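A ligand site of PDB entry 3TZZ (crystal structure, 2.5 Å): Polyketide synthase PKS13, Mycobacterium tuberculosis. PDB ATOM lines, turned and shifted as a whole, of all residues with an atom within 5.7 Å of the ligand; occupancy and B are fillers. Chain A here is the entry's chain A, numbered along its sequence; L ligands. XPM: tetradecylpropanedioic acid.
The side-chain hydroxyl of Ser 230 is covalently linked to a carbon (C1) of the ligand, at 1.3 Å. An oxygen (O2) of the ligand sits close to the backbone NH (N) of Leu 231 (3.3 Å). OG of Ser 337 lies within hydrogen-bond range of O2B of the ligand (3.1 Å). NE2 of His 338 lies within hydrogen-bond range of O2B of the ligand, 2.6 Å away. The guanidinium group of Arg 255 lies within salt-bridge range of an oxygen (O2A) of the ligand (2.6 Å).
SD of Met 274 is in hydrogen-bond range of N of Ser 337, at 3.7 Å. The backbone NH of Lys 334 is in hydrogen-bond range of the side-chain carboxylate of Glu 263 (2.8 Å). O of Gly 335 is in hydrogen-bond range of OG1 of Thr 333. O of Leu 266 is in hydrogen-bond range of NZ of Lys 334, at 2.5 Å. The side-chain hydroxyl of Ser 230 sits at hydrogen-bond distance from a ring nitrogen (NE2) of His 338. SD of Met 259 sits at hydrogen-bond distance from NH1 of Arg 255 (3.7 Å). The backbone NH (N) of Ala 336 is in hydrogen-bond range of the side-chain amide oxygen (OE1) of Gln 341 (2.7 Å). The backbone NH (N) of His 338 is in hydrogen-bond range of the backbone carbonyl oxygen (O) of Leu 392, 3.0 Å away.
CB of Phe 148 touches O2 of the ligand, at 3.2 Å. Gln 202 touches the ligand. O of Met 259 touches CB of the ligand, 3.3 Å away. Gly 262 touches the ligand (C to CE, 3.6 Å). CB of Glu 263 touches CB of the ligand, 3.7 Å away. CD1 of Leu 266 touches CC of the ligand, at 3.7 Å. Thr 333 touches the ligand. O of Gly 335 touches C8 of the ligand, 3.5 Å away. O of Gln 341 touches CF of the ligand (3.5 Å). Met 342 touches the ligand. Within 4 Å of the ligand: Phe 148, Gln 202, Ser 230, Leu 231, Arg 255, Met 259, Gly 262, Glu 263, Leu 266, Thr 333, Gly 335, Ser 337, His 338, Gln 341 and Met 342. The nearest printed residue that does not touch the ligand is Ala 336 (4.05 Å).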
ATOM      1  N   GLY A 147      28.288   0.563   6.405  1.00  0.00           N
ATOM      2  CA  GLY A 147      28.518   0.736   4.968  1.00  0.00           C
ATOM      3  C   GLY A 147      27.451   0.169   4.063  1.00  0.00           C
ATOM      4  O   GLY A 147      27.163   0.729   3.012  1.00  0.00           O
ATOM      5  N   PHE A 148      26.850  -0.947   4.466  1.00  0.00           N
ATOM      6  CA  PHE A 148      25.745  -1.493   3.700  1.00  0.00           C
ATOM      7  C   PHE A 148      24.702  -0.417   3.424  1.00  0.00           C
ATOM      8  O   PHE A 148      24.326   0.325   4.321  1.00  0.00           O
ATOM      9  CB  PHE A 148      25.062  -2.644   4.447  1.00  0.00           C
ATOM     10  CG  PHE A 148      24.112  -3.422   3.589  1.00  0.00           C
ATOM     11  CD1 PHE A 148      24.588  -4.346   2.659  1.00  0.00           C
ATOM     12  CD2 PHE A 148      22.730  -3.208   3.671  1.00  0.00           C
ATOM     13  CE1 PHE A 148      23.719  -5.063   1.845  1.00  0.00           C
ATOM     14  CE2 PHE A 148      21.859  -3.918   2.864  1.00  0.00           C
ATOM     15  CZ  PHE A 148      22.344  -4.845   1.950  1.00  0.00           C
ATOM     16  N   ILE A 198      28.952  -5.713  -5.640  1.00  0.00           N
ATOM     17  CA  ILE A 198      29.161  -6.273  -4.314  1.00  0.00           C
ATOM     18  C   ILE A 198      30.617  -6.091  -3.886  1.00  0.00           C
ATOM     19  O   ILE A 198      30.879  -5.540  -2.822  1.00  0.00           O
ATOM     20  CB  ILE A 198      28.706  -7.753  -4.236  1.00  0.00           C
ATOM     21  CG1 ILE A 198      27.164  -7.795  -4.181  1.00  0.00           C
ATOM     22  CG2 ILE A 198      29.324  -8.463  -3.032  1.00  0.00           C
ATOM     23  CD1 ILE A 198      26.557  -9.167  -4.326  1.00  0.00           C
ATOM     24  N   GLN A 202      32.472  -2.626  -1.247  1.00  0.00           N
ATOM     25  CA  GLN A 202      33.156  -2.881  -0.010  1.00  0.00           C
ATOM     26  C   GLN A 202      34.497  -2.184   0.042  1.00  0.00           C
ATOM     27  O   GLN A 202      34.752  -1.386   0.956  1.00  0.00           O
ATOM     28  CB  GLN A 202      33.319  -4.376   0.202  1.00  0.00           C
ATOM     29  CG  GLN A 202      32.006  -5.070   0.456  1.00  0.00           C
ATOM     30  CD  GLN A 202      32.194  -6.498   0.890  1.00  0.00           C
ATOM     31  OE1 GLN A 202      33.175  -6.845   1.549  1.00  0.00           O
ATOM     32  NE2 GLN A 202      31.251  -7.349   0.508  1.00  0.00           N
ATOM     33  N   GLN A 229      29.885  -2.511  11.609  1.00  0.00           N
ATOM     34  CA  GLN A 229      28.749  -3.264  11.076  1.00  0.00           C
ATOM     35  C   GLN A 229      29.162  -3.912   9.768  1.00  0.00           C
ATOM     36  O   GLN A 229      29.396  -3.226   8.760  1.00  0.00           O
ATOM     37  CB  GLN A 229      27.514  -2.387  10.894  1.00  0.00           C
ATOM     38  CG  GLN A 229      26.243  -3.167  10.654  1.00  0.00           C
ATOM     39  CD  GLN A 229      25.132  -2.298  10.089  1.00  0.00           C
ATOM     40  OE1 GLN A 229      25.155  -1.960   8.919  1.00  0.00           O
ATOM     41  NE2 GLN A 229      24.164  -1.926  10.924  1.00  0.00           N
ATOM     42  N   SER A 230      29.293  -5.235   9.815  1.00  0.00           N
ATOM     43  CA  SER A 230      29.420  -6.069   8.624  1.00  0.00           C
ATOM     44  C   SER A 230      30.639  -5.650   7.794  1.00  0.00           C
ATOM     45  O   SER A 230      31.791  -5.807   8.219  1.00  0.00           O
ATOM     46  CB  SER A 230      28.099  -6.013   7.824  1.00  0.00           C
ATOM     47  OG  SER A 230      28.183  -6.705   6.587  1.00  0.00           O
ATOM     48  N   LEU A 231      30.367  -5.084   6.631  1.00  0.00           N
ATOM     49  CA  LEU A 231      31.354  -4.494   5.756  1.00  0.00           C
ATOM     50  C   LEU A 231      32.382  -3.658   6.529  1.00  0.00           C
ATOM     51  O   LEU A 231      33.597  -3.870   6.408  1.00  0.00           O
ATOM     52  CB  LEU A 231      30.553  -3.632   4.792  1.00  0.00           C
ATOM     53  CG  LEU A 231      31.089  -2.803   3.666  1.00  0.00           C
ATOM     54  CD1 LEU A 231      30.001  -2.808   2.616  1.00  0.00           C
ATOM     55  CD2 LEU A 231      31.354  -1.404   4.163  1.00  0.00           C
ATOM     56  N   GLY A 232      31.878  -2.745   7.361  1.00  0.00           N
ATOM     57  CA  GLY A 232      32.720  -1.792   8.086  1.00  0.00           C
ATOM     58  C   GLY A 232      33.714  -2.325   9.107  1.00  0.00           C
ATOM     59  O   GLY A 232      34.522  -1.558   9.607  1.00  0.00           O
ATOM     60  N   ARG A 255      37.643 -10.724   1.744  1.00  0.00           N
ATOM     61  CA  ARG A 255      36.232 -11.016   1.867  1.00  0.00           C
ATOM     62  C   ARG A 255      35.410 -10.540   0.667  1.00  0.00           C
ATOM     63  O   ARG A 255      34.542 -11.261   0.190  1.00  0.00           O
ATOM     64  CB  ARG A 255      35.675 -10.492   3.181  1.00  0.00           C
ATOM     65  CG  ARG A 255      35.590  -8.986   3.283  1.00  0.00           C
ATOM     66  CD  ARG A 255      35.342  -8.553   4.722  1.00  0.00           C
ATOM     67  NE  ARG A 255      34.118  -9.101   5.292  1.00  0.00           N
ATOM     68  CZ  ARG A 255      32.880  -8.751   4.946  1.00  0.00           C
ATOM     69  NH1 ARG A 255      32.671  -7.863   3.972  1.00  0.00           N
ATOM     70  NH2 ARG A 255      31.833  -9.308   5.550  1.00  0.00           N
ATOM     71  N   LEU A 258      35.940 -12.636  -2.718  1.00  0.00           N
ATOM     72  CA  LEU A 258      35.398 -13.976  -2.514  1.00  0.00           C
ATOM     73  C   LEU A 258      33.888 -13.927  -2.484  1.00  0.00           C
ATOM     74  O   LEU A 258      33.228 -14.776  -3.075  1.00  0.00           O
ATOM     75  CB  LEU A 258      35.910 -14.606  -1.227  1.00  0.00           C
ATOM     76  CG  LEU A 258      37.398 -14.929  -1.193  1.00  0.00           C
ATOM     77  CD1 LEU A 258      37.835 -15.286   0.223  1.00  0.00           C
ATOM     78  CD2 LEU A 258      37.749 -16.023  -2.196  1.00  0.00           C
ATOM     79  N   MET A 259      33.334 -12.919  -1.818  1.00  0.00           N
ATOM     80  CA  MET A 259      31.893 -12.734  -1.768  1.00  0.00           C
ATOM     81  C   MET A 259      31.319 -12.356  -3.132  1.00  0.00           C
ATOM     82  O   MET A 259      30.314 -12.930  -3.548  1.00  0.00           O
ATOM     83  CB  MET A 259      31.528 -11.662  -0.748  1.00  0.00           C
ATOM     84  CG  MET A 259      31.901 -12.036   0.679  1.00  0.00           C
ATOM     85  SD  MET A 259      31.703 -10.675   1.843  1.00  0.00           S
ATOM     86  CE  MET A 259      29.933 -10.358   1.717  1.00  0.00           C
ATOM     87  N   GLY A 260      31.966 -11.386  -3.803  1.00  0.00           N
ATOM     88  CA  GLY A 260      31.514 -10.875  -5.089  1.00  0.00           C
ATOM     89  C   GLY A 260      31.597 -11.881  -6.225  1.00  0.00           C
ATOM     90  O   GLY A 260      30.696 -11.960  -7.066  1.00  0.00           O
ATOM     91  N   GLY A 262      31.734 -15.152  -5.635  1.00  0.00           N
ATOM     92  CA  GLY A 262      30.915 -16.282  -5.208  1.00  0.00           C
ATOM     93  C   GLY A 262      29.452 -16.072  -5.553  1.00  0.00           C
ATOM     94  O   GLY A 262      28.779 -16.987  -6.022  1.00  0.00           O
ATOM     95  N   GLU A 263      28.947 -14.863  -5.325  1.00  0.00           N
ATOM     96  CA  GLU A 263      27.532 -14.623  -5.562  1.00  0.00           C
ATOM     97  C   GLU A 263      27.183 -14.524  -7.039  1.00  0.00           C
ATOM     98  O   GLU A 263      26.054 -14.821  -7.412  1.00  0.00           O
ATOM     99  CB  GLU A 263      27.026 -13.430  -4.762  1.00  0.00           C
ATOM    100  CG  GLU A 263      27.071 -12.105  -5.477  1.00  0.00           C
ATOM    101  CD  GLU A 263      25.794 -11.807  -6.219  1.00  0.00           C
ATOM    102  OE1 GLU A 263      24.701 -12.009  -5.649  1.00  0.00           O
ATOM    103  OE2 GLU A 263      25.885 -11.361  -7.372  1.00  0.00           O
ATOM    104  N   LEU A 266      26.020 -17.838  -8.463  1.00  0.00           N
ATOM    105  CA  LEU A 266      24.867 -18.442  -7.786  1.00  0.00           C
ATOM    106  C   LEU A 266      23.575 -18.443  -8.614  1.00  0.00           C
ATOM    107  O   LEU A 266      23.083 -17.386  -8.996  1.00  0.00           O
ATOM    108  CB  LEU A 266      24.624 -17.753  -6.436  1.00  0.00           C
ATOM    109  CG  LEU A 266      25.635 -18.087  -5.335  1.00  0.00           C
ATOM    110  CD1 LEU A 266      25.352 -17.243  -4.110  1.00  0.00           C
ATOM    111  CD2 LEU A 266      25.579 -19.560  -4.997  1.00  0.00           C
ATOM    112  N   MET A 274      18.715 -11.991   1.103  1.00  0.00           N
ATOM    113  CA  MET A 274      18.788 -11.272   2.394  1.00  0.00           C
ATOM    114  C   MET A 274      17.651 -10.258   2.458  1.00  0.00           C
ATOM    115  O   MET A 274      17.320  -9.629   1.462  1.00  0.00           O
ATOM    116  CB  MET A 274      20.130 -10.539   2.534  1.00  0.00           C
ATOM    117  CG  MET A 274      21.343 -11.430   2.367  1.00  0.00           C
ATOM    118  SD  MET A 274      22.903 -10.554   2.556  1.00  0.00           S
ATOM    119  CE  MET A 274      22.909 -10.273   4.331  1.00  0.00           C
ATOM    120  N   THR A 333      20.720  -9.049  -3.842  1.00  0.00           N
ATOM    121  CA  THR A 333      21.806  -9.997  -3.794  1.00  0.00           C
ATOM    122  C   THR A 333      21.301 -11.411  -3.963  1.00  0.00           C
ATOM    123  O   THR A 333      20.181 -11.713  -3.547  1.00  0.00           O
ATOM    124  CB  THR A 333      22.614  -9.890  -2.493  1.00  0.00           C
ATOM    125  OG1 THR A 333      23.616 -10.907  -2.470  1.00  0.00           O
ATOM    126  CG2 THR A 333      21.700 -10.035  -1.284  1.00  0.00           C
ATOM    127  N   LYS A 334      22.115 -12.264  -4.587  1.00  0.00           N
ATOM    128  CA  LYS A 334      21.789 -13.680  -4.808  1.00  0.00           C
ATOM    129  C   LYS A 334      22.377 -14.605  -3.737  1.00  0.00           C
ATOM    130  O   LYS A 334      22.143 -15.816  -3.759  1.00  0.00           O
ATOM    131  CB  LYS A 334      22.240 -14.140  -6.197  1.00  0.00           C
ATOM    132  CG  LYS A 334      21.531 -13.462  -7.353  1.00  0.00           C
ATOM    133  CD  LYS A 334      22.364 -13.541  -8.625  1.00  0.00           C
ATOM    134  CE  LYS A 334      22.052 -14.793  -9.413  1.00  0.00           C
ATOM    135  NZ  LYS A 334      23.228 -15.189 -10.226  1.00  0.00           N
ATOM    136  N   GLY A 335      23.160 -14.025  -2.823  1.00  0.00           N
ATOM    137  CA  GLY A 335      23.759 -14.755  -1.708  1.00  0.00           C
ATOM    138  C   GLY A 335      23.605 -14.073  -0.346  1.00  0.00           C
ATOM    139  O   GLY A 335      23.557 -12.840  -0.243  1.00  0.00           O
ATOM    140  N   ALA A 336      23.538 -14.882   0.700  1.00  0.00           N
ATOM    141  CA  ALA A 336      23.368 -14.392   2.054  1.00  0.00           C
ATOM    142  C   ALA A 336      24.664 -14.496   2.855  1.00  0.00           C
ATOM    143  O   ALA A 336      25.044 -15.584   3.297  1.00  0.00           O
ATOM    144  CB  ALA A 336      22.248 -15.157   2.755  1.00  0.00           C
ATOM    145  N   SER A 337      25.312 -13.360   3.062  1.00  0.00           N
ATOM    146  CA  SER A 337      26.420 -13.298   4.011  1.00  0.00           C
ATOM    147  C   SER A 337      25.867 -13.508   5.420  1.00  0.00           C
ATOM    148  O   SER A 337      24.662 -13.355   5.646  1.00  0.00           O
ATOM    149  CB  SER A 337      27.149 -11.959   3.914  1.00  0.00           C
ATOM    150  OG  SER A 337      26.301 -10.921   4.388  1.00  0.00           O
ATOM    151  N   HIS A 338      26.746 -13.848   6.372  1.00  0.00           N
ATOM    152  CA  HIS A 338      26.372 -14.114   7.775  1.00  0.00           C
ATOM    153  C   HIS A 338      25.424 -15.278   7.944  1.00  0.00           C
ATOM    154  O   HIS A 338      24.629 -15.304   8.885  1.00  0.00           O
ATOM    155  CB  HIS A 338      25.886 -12.844   8.482  1.00  0.00           C
ATOM    156  CG  HIS A 338      26.801 -11.666   8.259  1.00  0.00           C
ATOM    157  ND1 HIS A 338      28.051 -11.603   8.778  1.00  0.00           N
ATOM    158  CD2 HIS A 338      26.636 -10.513   7.495  1.00  0.00           C
ATOM    159  CE1 HIS A 338      28.644 -10.478   8.367  1.00  0.00           C
ATOM    160  NE2 HIS A 338      27.779  -9.804   7.589  1.00  0.00           N
ATOM    161  N   GLN A 341      25.681 -20.591   4.212  1.00  0.00           N
ATOM    162  CA  GLN A 341      26.114 -20.493   2.800  1.00  0.00           C
ATOM    163  C   GLN A 341      27.577 -20.137   2.639  1.00  0.00           C
ATOM    164  O   GLN A 341      28.210 -20.462   1.622  1.00  0.00           O
ATOM    165  CB  GLN A 341      25.286 -19.447   2.059  1.00  0.00           C
ATOM    166  CG  GLN A 341      25.553 -19.415   0.561  1.00  0.00           C
ATOM    167  CD  GLN A 341      24.638 -18.475  -0.200  1.00  0.00           C
ATOM    168  OE1 GLN A 341      24.346 -17.371   0.253  1.00  0.00           O
ATOM    169  NE2 GLN A 341      24.185 -18.912  -1.349  1.00  0.00           N
ATOM    170  N   MET A 342      28.112 -19.452   3.644  1.00  0.00           N
ATOM    171  CA  MET A 342      29.434 -18.850   3.565  1.00  0.00           C
ATOM    172  C   MET A 342      30.561 -19.857   3.786  1.00  0.00           C
ATOM    173  O   MET A 342      31.719 -19.585   3.438  1.00  0.00           O
ATOM    174  CB  MET A 342      29.496 -17.694   4.553  1.00  0.00           C
ATOM    175  CG  MET A 342      29.982 -16.416   3.922  1.00  0.00           C
ATOM    176  SD  MET A 342      28.711 -15.542   2.983  1.00  0.00           S
ATOM    177  CE  MET A 342      28.351 -16.646   1.624  1.00  0.00           C
ATOM    178  N   PRO A 344      31.832 -22.504   2.272  1.00  0.00           N
ATOM    179  CA  PRO A 344      32.807 -22.802   1.215  1.00  0.00           C
ATOM    180  C   PRO A 344      33.876 -21.715   1.001  1.00  0.00           C
ATOM    181  O   PRO A 344      34.927 -21.993   0.422  1.00  0.00           O
ATOM    182  CB  PRO A 344      31.943 -22.902  -0.044  1.00  0.00           C
ATOM    183  CG  PRO A 344      30.569 -23.205   0.449  1.00  0.00           C
ATOM    184  CD  PRO A 344      30.456 -22.480   1.762  1.00  0.00           C
ATOM    185  N   LEU A 345      33.594 -20.498   1.449  1.00  0.00           N
ATOM    186  CA  LEU A 345      34.545 -19.413   1.282  1.00  0.00           C
ATOM    187  C   LEU A 345      35.627 -19.437   2.357  1.00  0.00           C
ATOM    188  O   LEU A 345      36.726 -18.935   2.137  1.00  0.00           O
ATOM    189  CB  LEU A 345      33.846 -18.054   1.326  1.00  0.00           C
ATOM    190  CG  LEU A 345      32.649 -17.758   0.445  1.00  0.00           C
ATOM    191  CD1 LEU A 345      32.485 -16.248   0.392  1.00  0.00           C
ATOM    192  CD2 LEU A 345      32.846 -18.341  -0.947  1.00  0.00           C
ATOM    193  N   LEU A 392      32.395 -13.184   8.914  1.00  0.00           N
ATOM    194  CA  LEU A 392      31.675 -13.532   7.695  1.00  0.00           C
ATOM    195  C   LEU A 392      30.600 -14.603   7.895  1.00  0.00           C
ATOM    196  O   LEU A 392      29.459 -14.419   7.473  1.00  0.00           O
ATOM    197  CB  LEU A 392      32.672 -13.952   6.626  1.00  0.00           C
ATOM    198  CG  LEU A 392      32.164 -14.200   5.202  1.00  0.00           C
ATOM    199  CD1 LEU A 392      31.444 -13.009   4.580  1.00  0.00           C
ATOM    200  CD2 LEU A 392      33.371 -14.599   4.379  1.00  0.00           C
HETATM  201  C1  XPM L   1      27.862  -6.053   5.465  1.00  0.00           C
HETATM  202  C2  XPM L   1      28.055  -6.857   4.187  1.00  0.00           C
HETATM  203  O2  XPM L   1      27.447  -4.738   5.062  1.00  0.00           O
HETATM  204  C3  XPM L   1      26.739  -7.191   3.461  1.00  0.00           C
HETATM  205  C4  XPM L   1      26.907  -7.050   1.941  1.00  0.00           C
HETATM  206  C5  XPM L   1      25.941  -7.969   1.178  1.00  0.00           C
HETATM  207  C6  XPM L   1      26.668  -8.789   0.121  1.00  0.00           C
HETATM  208  C7  XPM L   1      25.908 -10.067  -0.169  1.00  0.00           C
HETATM  209  C8  XPM L   1      26.653 -11.300   0.317  1.00  0.00           C
HETATM  210  C9  XPM L   1      27.312 -12.035  -0.845  1.00  0.00           C
HETATM  211  CA  XPM L   1      27.043 -13.539  -0.813  1.00  0.00           C
HETATM  212  CB  XPM L   1      28.234 -14.284  -1.374  1.00  0.00           C
HETATM  213  CC  XPM L   1      27.864 -15.677  -1.843  1.00  0.00           C
HETATM  214  CD  XPM L   1      29.070 -16.594  -1.762  1.00  0.00           C
HETATM  215  CE  XPM L   1      28.803 -17.912  -2.476  1.00  0.00           C
HETATM  216  CF  XPM L   1      28.803 -19.078  -1.486  1.00  0.00           C
HETATM  217  CG  XPM L   1      28.790 -20.407  -2.214  1.00  0.00           C
HETATM  218  C2A XPM L   1      28.926  -8.039   4.531  1.00  0.00           C
HETATM  219  O2A XPM L   1      30.071  -7.971   4.081  1.00  0.00           O
HETATM  220  O2B XPM L   1      28.528  -8.969   5.262  1.00  0.00           O
